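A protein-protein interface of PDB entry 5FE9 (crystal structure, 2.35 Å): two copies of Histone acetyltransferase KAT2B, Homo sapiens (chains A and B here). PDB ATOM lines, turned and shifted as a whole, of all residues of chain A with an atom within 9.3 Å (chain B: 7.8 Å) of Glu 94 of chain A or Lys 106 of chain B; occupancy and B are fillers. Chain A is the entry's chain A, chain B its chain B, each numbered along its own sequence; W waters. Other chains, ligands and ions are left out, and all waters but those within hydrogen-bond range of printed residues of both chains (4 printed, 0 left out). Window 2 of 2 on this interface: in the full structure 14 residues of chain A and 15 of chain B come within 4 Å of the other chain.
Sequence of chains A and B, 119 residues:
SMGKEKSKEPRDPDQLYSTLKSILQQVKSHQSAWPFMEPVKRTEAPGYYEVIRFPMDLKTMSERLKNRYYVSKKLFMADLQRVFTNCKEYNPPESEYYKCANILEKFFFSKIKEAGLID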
ATOM      1  N   CYS A  87     -12.415   8.387 -22.871  1.00  0.00           N
ATOM      2  CA  CYS A  87     -12.674   7.033 -23.311  1.00  0.00           C
ATOM      3  C   CYS A  87     -14.014   6.913 -24.041  1.00  0.00           C
ATOM      4  O   CYS A  87     -14.100   6.259 -25.089  1.00  0.00           O
ATOM      5  CB  CYS A  87     -12.652   6.104 -22.100  1.00  0.00           C
ATOM      6  SG  CYS A  87     -12.950   4.387 -22.526  1.00  0.00           S
ATOM      7  N   LYS A  88     -15.052   7.550 -23.501  1.00  0.00           N
ATOM      8  CA  LYS A  88     -16.368   7.427 -24.080  1.00  0.00           C
ATOM      9  C   LYS A  88     -16.501   8.173 -25.381  1.00  0.00           C
ATOM     10  O   LYS A  88     -17.261   7.711 -26.260  1.00  0.00           O
ATOM     11  CB  LYS A  88     -17.435   7.844 -23.089  1.00  0.00           C
ATOM     12  CG  LYS A  88     -17.534   6.850 -21.973  1.00  0.00           C
ATOM     13  CD  LYS A  88     -18.775   7.037 -21.086  1.00  0.00           C
ATOM     14  CE  LYS A  88     -18.400   7.596 -19.748  1.00  0.00           C
ATOM     15  NZ  LYS A  88     -19.577   7.841 -18.896  1.00  0.00           N
ATOM     16  N   GLU A  89     -15.796   9.311 -25.510  1.00  0.00           N
ATOM     17  CA  GLU A  89     -15.806  10.062 -26.794  1.00  0.00           C
ATOM     18  C   GLU A  89     -15.107   9.275 -27.897  1.00  0.00           C
ATOM     19  O   GLU A  89     -15.611   9.208 -29.021  1.00  0.00           O
ATOM     20  CB  GLU A  89     -15.225  11.509 -26.681  1.00  0.00           C
ATOM     21  CG  GLU A  89     -14.575  12.118 -27.942  1.00  0.00           C
ATOM     22  CD  GLU A  89     -14.767  13.643 -28.000  1.00  0.00           C
ATOM     23  OE1 GLU A  89     -14.499  14.276 -26.952  1.00  0.00           O
ATOM     24  OE2 GLU A  89     -15.190  14.204 -29.067  1.00  0.00           O
ATOM     25  N   ASN A  91     -14.101   5.878 -28.043  1.00  0.00           N
ATOM     26  CA  ASN A  91     -14.470   4.489 -28.342  1.00  0.00           C
ATOM     27  C   ASN A  91     -15.964   4.251 -28.662  1.00  0.00           C
ATOM     28  O   ASN A  91     -16.835   4.949 -28.128  1.00  0.00           O
ATOM     29  CB  ASN A  91     -14.078   3.623 -27.172  1.00  0.00           C
ATOM     30  CG  ASN A  91     -12.571   3.600 -26.955  1.00  0.00           C
ATOM     31  OD1 ASN A  91     -11.854   2.901 -27.649  1.00  0.00           O
ATOM     32  ND2 ASN A  91     -12.104   4.349 -25.979  1.00  0.00           N
ATOM     33  N   PRO A  92     -16.254   3.237 -29.512  1.00  0.00           N
ATOM     34  CA  PRO A  92     -17.657   2.885 -29.777  1.00  0.00           C
ATOM     35  C   PRO A  92     -18.336   2.311 -28.527  1.00  0.00           C
ATOM     36  O   PRO A  92     -17.652   1.740 -27.664  1.00  0.00           O
ATOM     37  CB  PRO A  92     -17.585   1.857 -30.913  1.00  0.00           C
ATOM     38  CG  PRO A  92     -16.164   1.394 -30.989  1.00  0.00           C
ATOM     39  CD  PRO A  92     -15.297   2.404 -30.286  1.00  0.00           C
ATOM     40  N   PRO A  93     -19.661   2.564 -28.384  1.00  0.00           N
ATOM     41  CA  PRO A  93     -20.381   2.431 -27.116  1.00  0.00           C
ATOM     42  C   PRO A  93     -20.441   1.012 -26.547  1.00  0.00           C
ATOM     43  O   PRO A  93     -20.546   0.843 -25.320  1.00  0.00           O
ATOM     44  CB  PRO A  93     -21.798   2.955 -27.446  1.00  0.00           C
ATOM     45  CG  PRO A  93     -21.915   2.918 -28.932  1.00  0.00           C
ATOM     46  CD  PRO A  93     -20.527   3.085 -29.466  1.00  0.00           C
ATOM     47  N   GLU A  94     -20.350   0.002 -27.413  1.00  0.00           N
ATOM     48  CA  GLU A  94     -20.357  -1.381 -26.947  1.00  0.00           C
ATOM     49  C   GLU A  94     -18.967  -1.981 -26.897  1.00  0.00           C
ATOM     50  O   GLU A  94     -18.837  -3.180 -26.697  1.00  0.00           O
ATOM     51  CB  GLU A  94     -21.332  -2.234 -27.786  1.00  0.00           C
ATOM     52  CG  GLU A  94     -22.743  -1.619 -27.940  1.00  0.00           C
ATOM     53  CD  GLU A  94     -23.409  -1.256 -26.603  1.00  0.00           C
ATOM     54  OE1 GLU A  94     -23.320  -2.068 -25.656  1.00  0.00           O
ATOM     55  OE2 GLU A  94     -24.016  -0.157 -26.493  1.00  0.00           O
ATOM     56  N   SER A  95     -17.931  -1.149 -27.025  1.00  0.00           N
ATOM     57  CA  SER A  95     -16.566  -1.607 -26.833  1.00  0.00           C
ATOM     58  C   SER A  95     -16.324  -1.930 -25.367  1.00  0.00           C
ATOM     59  O   SER A  95     -16.933  -1.335 -24.481  1.00  0.00           O
ATOM     60  CB  SER A  95     -15.532  -0.569 -27.294  1.00  0.00           C
ATOM     61  OG  SER A  95     -15.499   0.520 -26.406  1.00  0.00           O
ATOM     62  N   GLU A  96     -15.418  -2.867 -25.138  1.00  0.00           N
ATOM     63  CA  GLU A  96     -14.934  -3.219 -23.815  1.00  0.00           C
ATOM     64  C   GLU A  96     -14.382  -1.985 -23.069  1.00  0.00           C
ATOM     65  O   GLU A  96     -14.576  -1.851 -21.858  1.00  0.00           O
ATOM     66  CB  GLU A  96     -13.809  -4.274 -23.974  1.00  0.00           C
ATOM     67  CG  GLU A  96     -13.402  -5.065 -22.755  1.00  0.00           C
ATOM     68  CD  GLU A  96     -12.304  -6.073 -23.083  1.00  0.00           C
ATOM     69  OE1 GLU A  96     -11.397  -5.767 -23.924  1.00  0.00           O
ATOM     70  OE2 GLU A  96     -12.390  -7.191 -22.538  1.00  0.00           O
ATOM     71  N   TYR A  97     -13.710  -1.078 -23.788  1.00  0.00           N
ATOM     72  CA  TYR A  97     -13.175   0.145 -23.155  1.00  0.00           C
ATOM     73  C   TYR A  97     -14.294   1.028 -22.623  1.00  0.00           C
ATOM     74  O   TYR A  97     -14.194   1.523 -21.502  1.00  0.00           O
ATOM     75  CB  TYR A  97     -12.281   0.948 -24.108  1.00  0.00           C
ATOM     76  CG  TYR A  97     -11.019   0.224 -24.522  1.00  0.00           C
ATOM     77  CD1 TYR A  97     -10.182  -0.352 -23.587  1.00  0.00           C
ATOM     78  CD2 TYR A  97     -10.657   0.131 -25.860  1.00  0.00           C
ATOM     79  CE1 TYR A  97      -9.017  -1.001 -23.966  1.00  0.00           C
ATOM     80  CE2 TYR A  97      -9.497  -0.518 -26.250  1.00  0.00           C
ATOM     81  CZ  TYR A  97      -8.683  -1.074 -25.296  1.00  0.00           C
ATOM     82  OH  TYR A  97      -7.546  -1.719 -25.678  1.00  0.00           O
ATOM     83  N   TYR A  98     -15.337   1.237 -23.439  1.00  0.00           N
ATOM     84  CA  TYR A  98     -16.492   2.050 -23.037  1.00  0.00           C
ATOM     85  C   TYR A  98     -17.210   1.401 -21.855  1.00  0.00           C
ATOM     86  O   TYR A  98     -17.486   2.071 -20.888  1.00  0.00           O
ATOM     87  CB  TYR A  98     -17.451   2.259 -24.217  1.00  0.00           C
ATOM     88  CG  TYR A  98     -18.427   3.414 -24.076  1.00  0.00           C
ATOM     89  CD1 TYR A  98     -19.420   3.394 -23.107  1.00  0.00           C
ATOM     90  CD2 TYR A  98     -18.350   4.527 -24.911  1.00  0.00           C
ATOM     91  CE1 TYR A  98     -20.328   4.444 -22.983  1.00  0.00           C
ATOM     92  CE2 TYR A  98     -19.253   5.585 -24.787  1.00  0.00           C
ATOM     93  CZ  TYR A  98     -20.241   5.527 -23.827  1.00  0.00           C
ATOM     94  OH  TYR A  98     -21.130   6.546 -23.672  1.00  0.00           O
ATOM     95  N   LYS A  99     -17.413   0.088 -21.906  1.00  0.00           N
ATOM     96  CA  LYS A  99     -17.989  -0.659 -20.762  1.00  0.00           C
ATOM     97  C   LYS A  99     -17.212  -0.472 -19.458  1.00  0.00           C
ATOM     98  O   LYS A  99     -17.796  -0.151 -18.416  1.00  0.00           O
ATOM     99  CB  LYS A  99     -18.060  -2.153 -21.064  1.00  0.00           C
ATOM    100  CG  LYS A  99     -19.157  -2.518 -22.044  1.00  0.00           C
ATOM    101  CD  LYS A  99     -19.087  -3.997 -22.406  1.00  0.00           C
ATOM    102  CE  LYS A  99     -19.950  -4.287 -23.621  1.00  0.00           C
ATOM    103  NZ  LYS A  99     -19.411  -5.471 -24.336  1.00  0.00           N
ATOM    104  N   CYS A 100     -15.893  -0.677 -19.517  1.00  0.00           N
ATOM    105  CA  CYS A 100     -15.029  -0.476 -18.343  1.00  0.00           C
ATOM    106  C   CYS A 100     -15.194   0.933 -17.771  1.00  0.00           C
ATOM    107  O   CYS A 100     -15.296   1.100 -16.555  1.00  0.00           O
ATOM    108  CB  CYS A 100     -13.533  -0.743 -18.675  1.00  0.00           C
ATOM    109  SG  CYS A 100     -13.143  -2.495 -18.910  1.00  0.00           S
ATOM    110  N   ASN A 102     -17.715   3.031 -17.800  1.00  0.00           N
ATOM    111  CA  ASN A 102     -18.954   3.253 -17.056  1.00  0.00           C
ATOM    112  C   ASN A 102     -19.046   2.467 -15.785  1.00  0.00           C
ATOM    113  O   ASN A 102     -19.583   2.964 -14.811  1.00  0.00           O
ATOM    114  CB  ASN A 102     -20.176   2.988 -17.914  1.00  0.00           C
ATOM    115  CG  ASN A 102     -20.572   4.200 -18.726  1.00  0.00           C
ATOM    116  OD1 ASN A 102     -20.193   5.341 -18.405  1.00  0.00           O
ATOM    117  ND2 ASN A 102     -21.386   3.972 -19.767  1.00  0.00           N
ATOM    118  N   HIS B  30     -34.606  12.013 -28.375  1.00  0.00           N
ATOM    119  CA  HIS B  30     -34.321  10.670 -27.876  1.00  0.00           C
ATOM    120  C   HIS B  30     -35.268  10.310 -26.671  1.00  0.00           C
ATOM    121  O   HIS B  30     -35.565  11.166 -25.852  1.00  0.00           O
ATOM    122  CB  HIS B  30     -32.839  10.582 -27.468  1.00  0.00           C
ATOM    123  CG  HIS B  30     -32.325   9.191 -27.365  1.00  0.00           C
ATOM    124  ND1 HIS B  30     -32.481   8.423 -26.245  1.00  0.00           N
ATOM    125  CD2 HIS B  30     -31.653   8.416 -28.252  1.00  0.00           C
ATOM    126  CE1 HIS B  30     -31.944   7.232 -26.434  1.00  0.00           C
ATOM    127  NE2 HIS B  30     -31.432   7.199 -27.648  1.00  0.00           N
ATOM    128  N   PHE B  84     -24.989  15.397 -17.731  1.00  0.00           N
ATOM    129  CA  PHE B  84     -24.792  13.981 -17.359  1.00  0.00           C
ATOM    130  C   PHE B  84     -24.107  13.862 -16.015  1.00  0.00           C
ATOM    131  O   PHE B  84     -24.543  13.108 -15.180  1.00  0.00           O
ATOM    132  CB  PHE B  84     -24.034  13.196 -18.449  1.00  0.00           C
ATOM    133  CG  PHE B  84     -24.683  13.257 -19.833  1.00  0.00           C
ATOM    134  CD1 PHE B  84     -26.061  13.116 -19.983  1.00  0.00           C
ATOM    135  CD2 PHE B  84     -23.924  13.431 -20.994  1.00  0.00           C
ATOM    136  CE1 PHE B  84     -26.662  13.169 -21.235  1.00  0.00           C
ATOM    137  CE2 PHE B  84     -24.527  13.486 -22.252  1.00  0.00           C
ATOM    138  CZ  PHE B  84     -25.883  13.367 -22.374  1.00  0.00           C
ATOM    139  N   CYS B 100     -30.849   6.687 -17.759  1.00  0.00           N
ATOM    140  CA  CYS B 100     -31.106   7.582 -18.893  1.00  0.00           C
ATOM    141  C   CYS B 100     -29.844   8.371 -19.293  1.00  0.00           C
ATOM    142  O   CYS B 100     -29.536   8.502 -20.477  1.00  0.00           O
ATOM    143  CB  CYS B 100     -32.263   8.564 -18.589  1.00  0.00           C
ATOM    144  SG  CYS B 100     -33.889   7.791 -18.581  1.00  0.00           S
ATOM    145  N   ALA B 101     -29.132   8.881 -18.308  1.00  0.00           N
ATOM    146  CA  ALA B 101     -27.966   9.698 -18.577  1.00  0.00           C
ATOM    147  C   ALA B 101     -26.920   8.942 -19.388  1.00  0.00           C
ATOM    148  O   ALA B 101     -26.303   9.520 -20.266  1.00  0.00           O
ATOM    149  CB  ALA B 101     -27.347  10.201 -17.261  1.00  0.00           C
ATOM    150  N   ASN B 102     -26.671   7.674 -19.041  1.00  0.00           N
ATOM    151  CA  ASN B 102     -25.655   6.877 -19.741  1.00  0.00           C
ATOM    152  C   ASN B 102     -26.112   6.420 -21.133  1.00  0.00           C
ATOM    153  O   ASN B 102     -25.320   6.376 -22.047  1.00  0.00           O
ATOM    154  CB  ASN B 102     -25.214   5.668 -18.913  1.00  0.00           C
ATOM    155  CG  ASN B 102     -24.051   5.980 -17.982  1.00  0.00           C
ATOM    156  OD1 ASN B 102     -23.316   6.964 -18.174  1.00  0.00           O
ATOM    157  ND2 ASN B 102     -23.852   5.110 -16.978  1.00  0.00           N
ATOM    158  N   ILE B 103     -27.383   6.097 -21.257  1.00  0.00           N
ATOM    159  CA  ILE B 103     -27.984   5.775 -22.559  1.00  0.00           C
ATOM    160  C   ILE B 103     -27.864   6.982 -23.500  1.00  0.00           C
ATOM    161  O   ILE B 103     -27.383   6.869 -24.594  1.00  0.00           O
ATOM    162  CB  ILE B 103     -29.463   5.343 -22.409  1.00  0.00           C
ATOM    163  CG1 ILE B 103     -29.546   3.982 -21.713  1.00  0.00           C
ATOM    164  CG2 ILE B 103     -30.137   5.232 -23.770  1.00  0.00           C
ATOM    165  CD1 ILE B 103     -30.971   3.549 -21.329  1.00  0.00           C
ATOM    166  N   LEU B 104     -28.237   8.138 -23.016  1.00  0.00           N
ATOM    167  CA  LEU B 104     -28.228   9.345 -23.833  1.00  0.00           C
ATOM    168  C   LEU B 104     -26.836   9.860 -24.118  1.00  0.00           C
ATOM    169  O   LEU B 104     -26.597  10.485 -25.139  1.00  0.00           O
ATOM    170  CB  LEU B 104     -29.076  10.432 -23.147  1.00  0.00           C
ATOM    171  CG  LEU B 104     -29.407  11.681 -23.982  1.00  0.00           C
ATOM    172  CD1 LEU B 104     -30.265  11.298 -25.184  1.00  0.00           C
ATOM    173  CD2 LEU B 104     -30.082  12.764 -23.128  1.00  0.00           C
ATOM    174  N   GLU B 105     -25.929   9.653 -23.172  1.00  0.00           N
ATOM    175  CA  GLU B 105     -24.519   9.948 -23.392  1.00  0.00           C
ATOM    176  C   GLU B 105     -23.938   9.116 -24.522  1.00  0.00           C
ATOM    177  O   GLU B 105     -23.181   9.626 -25.337  1.00  0.00           O
ATOM    178  CB  GLU B 105     -23.732   9.720 -22.119  1.00  0.00           C
ATOM    179  CG  GLU B 105     -22.275  10.130 -22.221  1.00  0.00           C
ATOM    180  CD  GLU B 105     -21.519   9.790 -20.974  1.00  0.00           C
ATOM    181  OE1 GLU B 105     -21.754   8.711 -20.432  1.00  0.00           O
ATOM    182  OE2 GLU B 105     -20.635  10.587 -20.551  1.00  0.00           O
ATOM    183  N   LYS B 106     -24.228   7.827 -24.531  1.00  0.00           N
ATOM    184  CA  LYS B 106     -23.817   6.966 -25.637  1.00  0.00           C
ATOM    185  C   LYS B 106     -24.312   7.536 -26.963  1.00  0.00           C
ATOM    186  O   LYS B 106     -23.604   7.563 -27.949  1.00  0.00           O
ATOM    187  CB  LYS B 106     -24.401   5.570 -25.472  1.00  0.00           C
ATOM    188  CG  LYS B 106     -23.641   4.641 -24.565  1.00  0.00           C
ATOM    189  CD  LYS B 106     -24.156   3.218 -24.718  1.00  0.00           C
ATOM    190  CE  LYS B 106     -23.687   2.336 -23.578  1.00  0.00           C
ATOM    191  NZ  LYS B 106     -24.222   0.949 -23.706  1.00  0.00           N
ATOM    192  N   PHE B 107     -25.578   7.911 -26.986  1.00  0.00           N
ATOM    193  CA  PHE B 107     -26.209   8.398 -28.195  1.00  0.00           C
ATOM    194  C   PHE B 107     -25.529   9.688 -28.654  1.00  0.00           C
ATOM    195  O   PHE B 107     -25.082   9.800 -29.789  1.00  0.00           O
ATOM    196  CB  PHE B 107     -27.694   8.624 -27.931  1.00  0.00           C
ATOM    197  CG  PHE B 107     -28.435   9.131 -29.113  1.00  0.00           C
ATOM    198  CD1 PHE B 107     -28.778   8.276 -30.150  1.00  0.00           C
ATOM    199  CD2 PHE B 107     -28.766  10.495 -29.220  1.00  0.00           C
ATOM    200  CE1 PHE B 107     -29.492   8.747 -31.271  1.00  0.00           C
ATOM    201  CE2 PHE B 107     -29.477  10.967 -30.325  1.00  0.00           C
ATOM    202  CZ  PHE B 107     -29.838  10.090 -31.354  1.00  0.00           C
ATOM    203  N   PHE B 108     -25.407  10.615 -27.720  1.00  0.00           N
ATOM    204  CA  PHE B 108     -24.626  11.835 -27.884  1.00  0.00           C
ATOM    205  C   PHE B 108     -23.277  11.597 -28.543  1.00  0.00           C
ATOM    206  O   PHE B 108     -22.974  12.191 -29.580  1.00  0.00           O
ATOM    207  CB  PHE B 108     -24.486  12.498 -26.523  1.00  0.00           C
ATOM    208  CG  PHE B 108     -23.389  13.506 -26.431  1.00  0.00           C
ATOM    209  CD1 PHE B 108     -23.433  14.692 -27.161  1.00  0.00           C
ATOM    210  CD2 PHE B 108     -22.338  13.326 -25.510  1.00  0.00           C
ATOM    211  CE1 PHE B 108     -22.451  15.663 -26.992  1.00  0.00           C
ATOM    212  CE2 PHE B 108     -21.365  14.296 -25.337  1.00  0.00           C
ATOM    213  CZ  PHE B 108     -21.413  15.459 -26.094  1.00  0.00           C
ATOM    214  N   PHE B 109     -22.465  10.713 -27.974  1.00  0.00           N
ATOM    215  CA  PHE B 109     -21.135  10.506 -28.531  1.00  0.00           C
ATOM    216  C   PHE B 109     -21.186   9.913 -29.935  1.00  0.00           C
ATOM    217  O   PHE B 109     -20.312  10.195 -30.742  1.00  0.00           O
ATOM    218  CB  PHE B 109     -20.259   9.668 -27.597  1.00  0.00           C
ATOM    219  CG  PHE B 109     -19.768  10.426 -26.389  1.00  0.00           C
ATOM    220  CD1 PHE B 109     -19.053  11.589 -26.534  1.00  0.00           C
ATOM    221  CD2 PHE B 109     -19.969   9.927 -25.101  1.00  0.00           C
ATOM    222  CE1 PHE B 109     -18.573  12.271 -25.424  1.00  0.00           C
ATOM    223  CE2 PHE B 109     -19.479  10.596 -23.986  1.00  0.00           C
ATOM    224  CZ  PHE B 109     -18.796  11.777 -24.148  1.00  0.00           C
ATOM    225  N   SER B 110     -22.178   9.060 -30.210  1.00  0.00           N
ATOM    226  CA  SER B 110     -22.311   8.503 -31.568  1.00  0.00           C
ATOM    227  C   SER B 110     -22.648   9.617 -32.557  1.00  0.00           C
ATOM    228  O   SER B 110     -22.058   9.676 -33.596  1.00  0.00           O
ATOM    229  CB  SER B 110     -23.314   7.357 -31.632  1.00  0.00           C
ATOM    230  OG  SER B 110     -24.645   7.849 -31.570  1.00  0.00           O
ATOM    231  N   LYS B 111     -23.513  10.556 -32.172  1.00  0.00           N
ATOM    232  CA  LYS B 111     -23.843  11.692 -33.046  1.00  0.00           C
ATOM    233  C   LYS B 111     -22.719  12.701 -33.253  1.00  0.00           C
ATOM    234  O   LYS B 111     -22.531  13.166 -34.353  1.00  0.00           O
ATOM    235  CB  LYS B 111     -25.109  12.417 -32.573  1.00  0.00           C
ATOM    236  CG  LYS B 111     -26.356  11.566 -32.595  1.00  0.00           C
ATOM    237  CD  LYS B 111     -26.695  11.098 -33.991  1.00  0.00           C
ATOM    238  CE  LYS B 111     -27.680   9.955 -33.986  1.00  0.00           C
ATOM    239  NZ  LYS B 111     -27.936   9.437 -35.353  1.00  0.00           N
ATOM    240  N   ILE B 112     -21.987  13.029 -32.200  1.00  0.00           N
ATOM    241  CA  ILE B 112     -20.743  13.825 -32.291  1.00  0.00           C
ATOM    242  C   ILE B 112     -19.754  13.228 -33.322  1.00  0.00           C
ATOM    243  O   ILE B 112     -19.170  13.936 -34.146  1.00  0.00           O
ATOM    244  CB  ILE B 112     -20.057  13.909 -30.889  1.00  0.00           C
ATOM    245  CG1 ILE B 112     -20.875  14.769 -29.910  1.00  0.00           C
ATOM    246  CG2 ILE B 112     -18.624  14.430 -30.965  1.00  0.00           C
ATOM    247  CD1 ILE B 112     -20.867  16.252 -30.214  1.00  0.00           C
HETATM  248  O   HOH W   1     -21.689  -0.378 -22.939  1.00  0.00           O
HETATM  249  O   HOH W   2     -21.388   5.281 -14.983  1.00  0.00           O
HETATM  250  O   HOH W   3     -17.553  10.891 -30.353  1.00  0.00           O
HETATM  251  O   HOH W   4     -22.474   6.445 -21.502  1.00  0.00           O
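Printed residues of chain B within 4 Å of Lys 88 of chain A: Asn 102, Glu 105 and Phe 109.
Printed residues of chain B within 4 Å of Glu 89 of chain A: Phe 109 and Ile 112.
Of chain B, only Lys 106 comes within 4 Å of Pro 93 of chain A.
Printed residues of chain B within 4 Å of Glu 94 of chain A: Lys 106.
Of the printed residues of chain B, Asn 102 of chain A touches Asn 102 (3.5 Å).
Leu 104 of chain B touches none of the printed residues of chain A.
Of the printed residues of chain A, Glu 105 of chain B touches Lys 88 (2.8 Å) and Tyr 98 (3.9 Å).
Lys 106 of chain B touches just these residues of chain A: Pro 93 (3.6 Å), Glu 94 (3.0 Å) and Tyr 98 (3.3 Å).
Of the printed residues of chain A, Ile 112 of chain B touches Glu 89 (3.9 Å).
The nearest printed residue of chain B that does not touch Glu 94 of chain A is Asn 102 of chain B (8.0 Å).
The side-chain amide oxygen of Asn 102 of chain B lies close to the side-chain carboxylate of Glu 105 of chain B.
O of Glu 94 of chain A sits at hydrogen-bond distance from NZ of Lys 99 of chain A (3.3 Å).
OG of Ser 95 of chain A sits at hydrogen-bond distance from N of Tyr 98 of chain A (3.1 Å).
The side-chain amide oxygen (OD1) of Asn 102 of chain A is in hydrogen-bond range of the side-chain amino group (NZ) of Lys 88 of chain A, 2.6 Å away.
Of the 14 printed residues of chain A, 6 touch a printed residue of chain B.
Hydrophobic or aromatic side chains of chain B within 4 Å of the printed part of chain A: Phe 109 and Ile 112.
Among the printed residues, 11 pairs touch across the chains.
Asn 102 of chain B touches its own counterpart, Asn 102 of chain A.
Of the 11 pairs that touch across the chains among the printed residues, 1 has its exchanged pair printed and touching as well.
NZ of Lys 88 of chain A is in salt-bridge range of OE1 of Glu 105 of chain B, at 2.8 Å.
OE2 of Glu 94 of chain A lies within salt-bridge range of NZ of Lys 106 of chain B (3.0 Å).
OH of Tyr 98 of chain A sits close to N of Lys 106 of chain B (3.5 Å).
Water W4 lies within hydrogen-bond range of OH of Tyr 98 of chain A, OE1 of Glu 105 of chain B, O of Asn 102 of chain B and ND2 of Asn 102 of chain A.
Water W3 lies within hydrogen-bond range of the backbone carbonyl oxygen (O) of Phe 109 of chain B (2.9 Å) and the backbone carbonyl oxygen (O) of Glu 89 of chain A (2.9 Å).
Water W1 bridges the backbone carbonyl oxygen (O) of Pro 93 of chain A (2.9 Å) and the side-chain amino group (NZ) of Lys 106 of chain B (3.0 Å).
Water W2 bridges O of Asn 102 of chain A (2.9 Å) and ND2 of Asn 102 of chain B (3.2 Å).
Lys 88 of chain A touches Asn 102 of chain B.
Lys 88 of chain A touches Phe 109 of chain B.
Glu 89 of chain A touches Phe 109 of chain B.
OE2 of Glu 89 of chain A touches CG2 of Ile 112 of chain B, 3.9 Å away.
CB of Pro 93 of chain A touches CD of Lys 106 of chain B (3.6 Å).
Glu 105 of chain B touches Tyr 98 of chain A (C to OH, 3.9 Å).
Phe 109 of chain B touches Tyr 98 of chain A.
Asn 102 of chain B touches Asn 102 of chain A.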
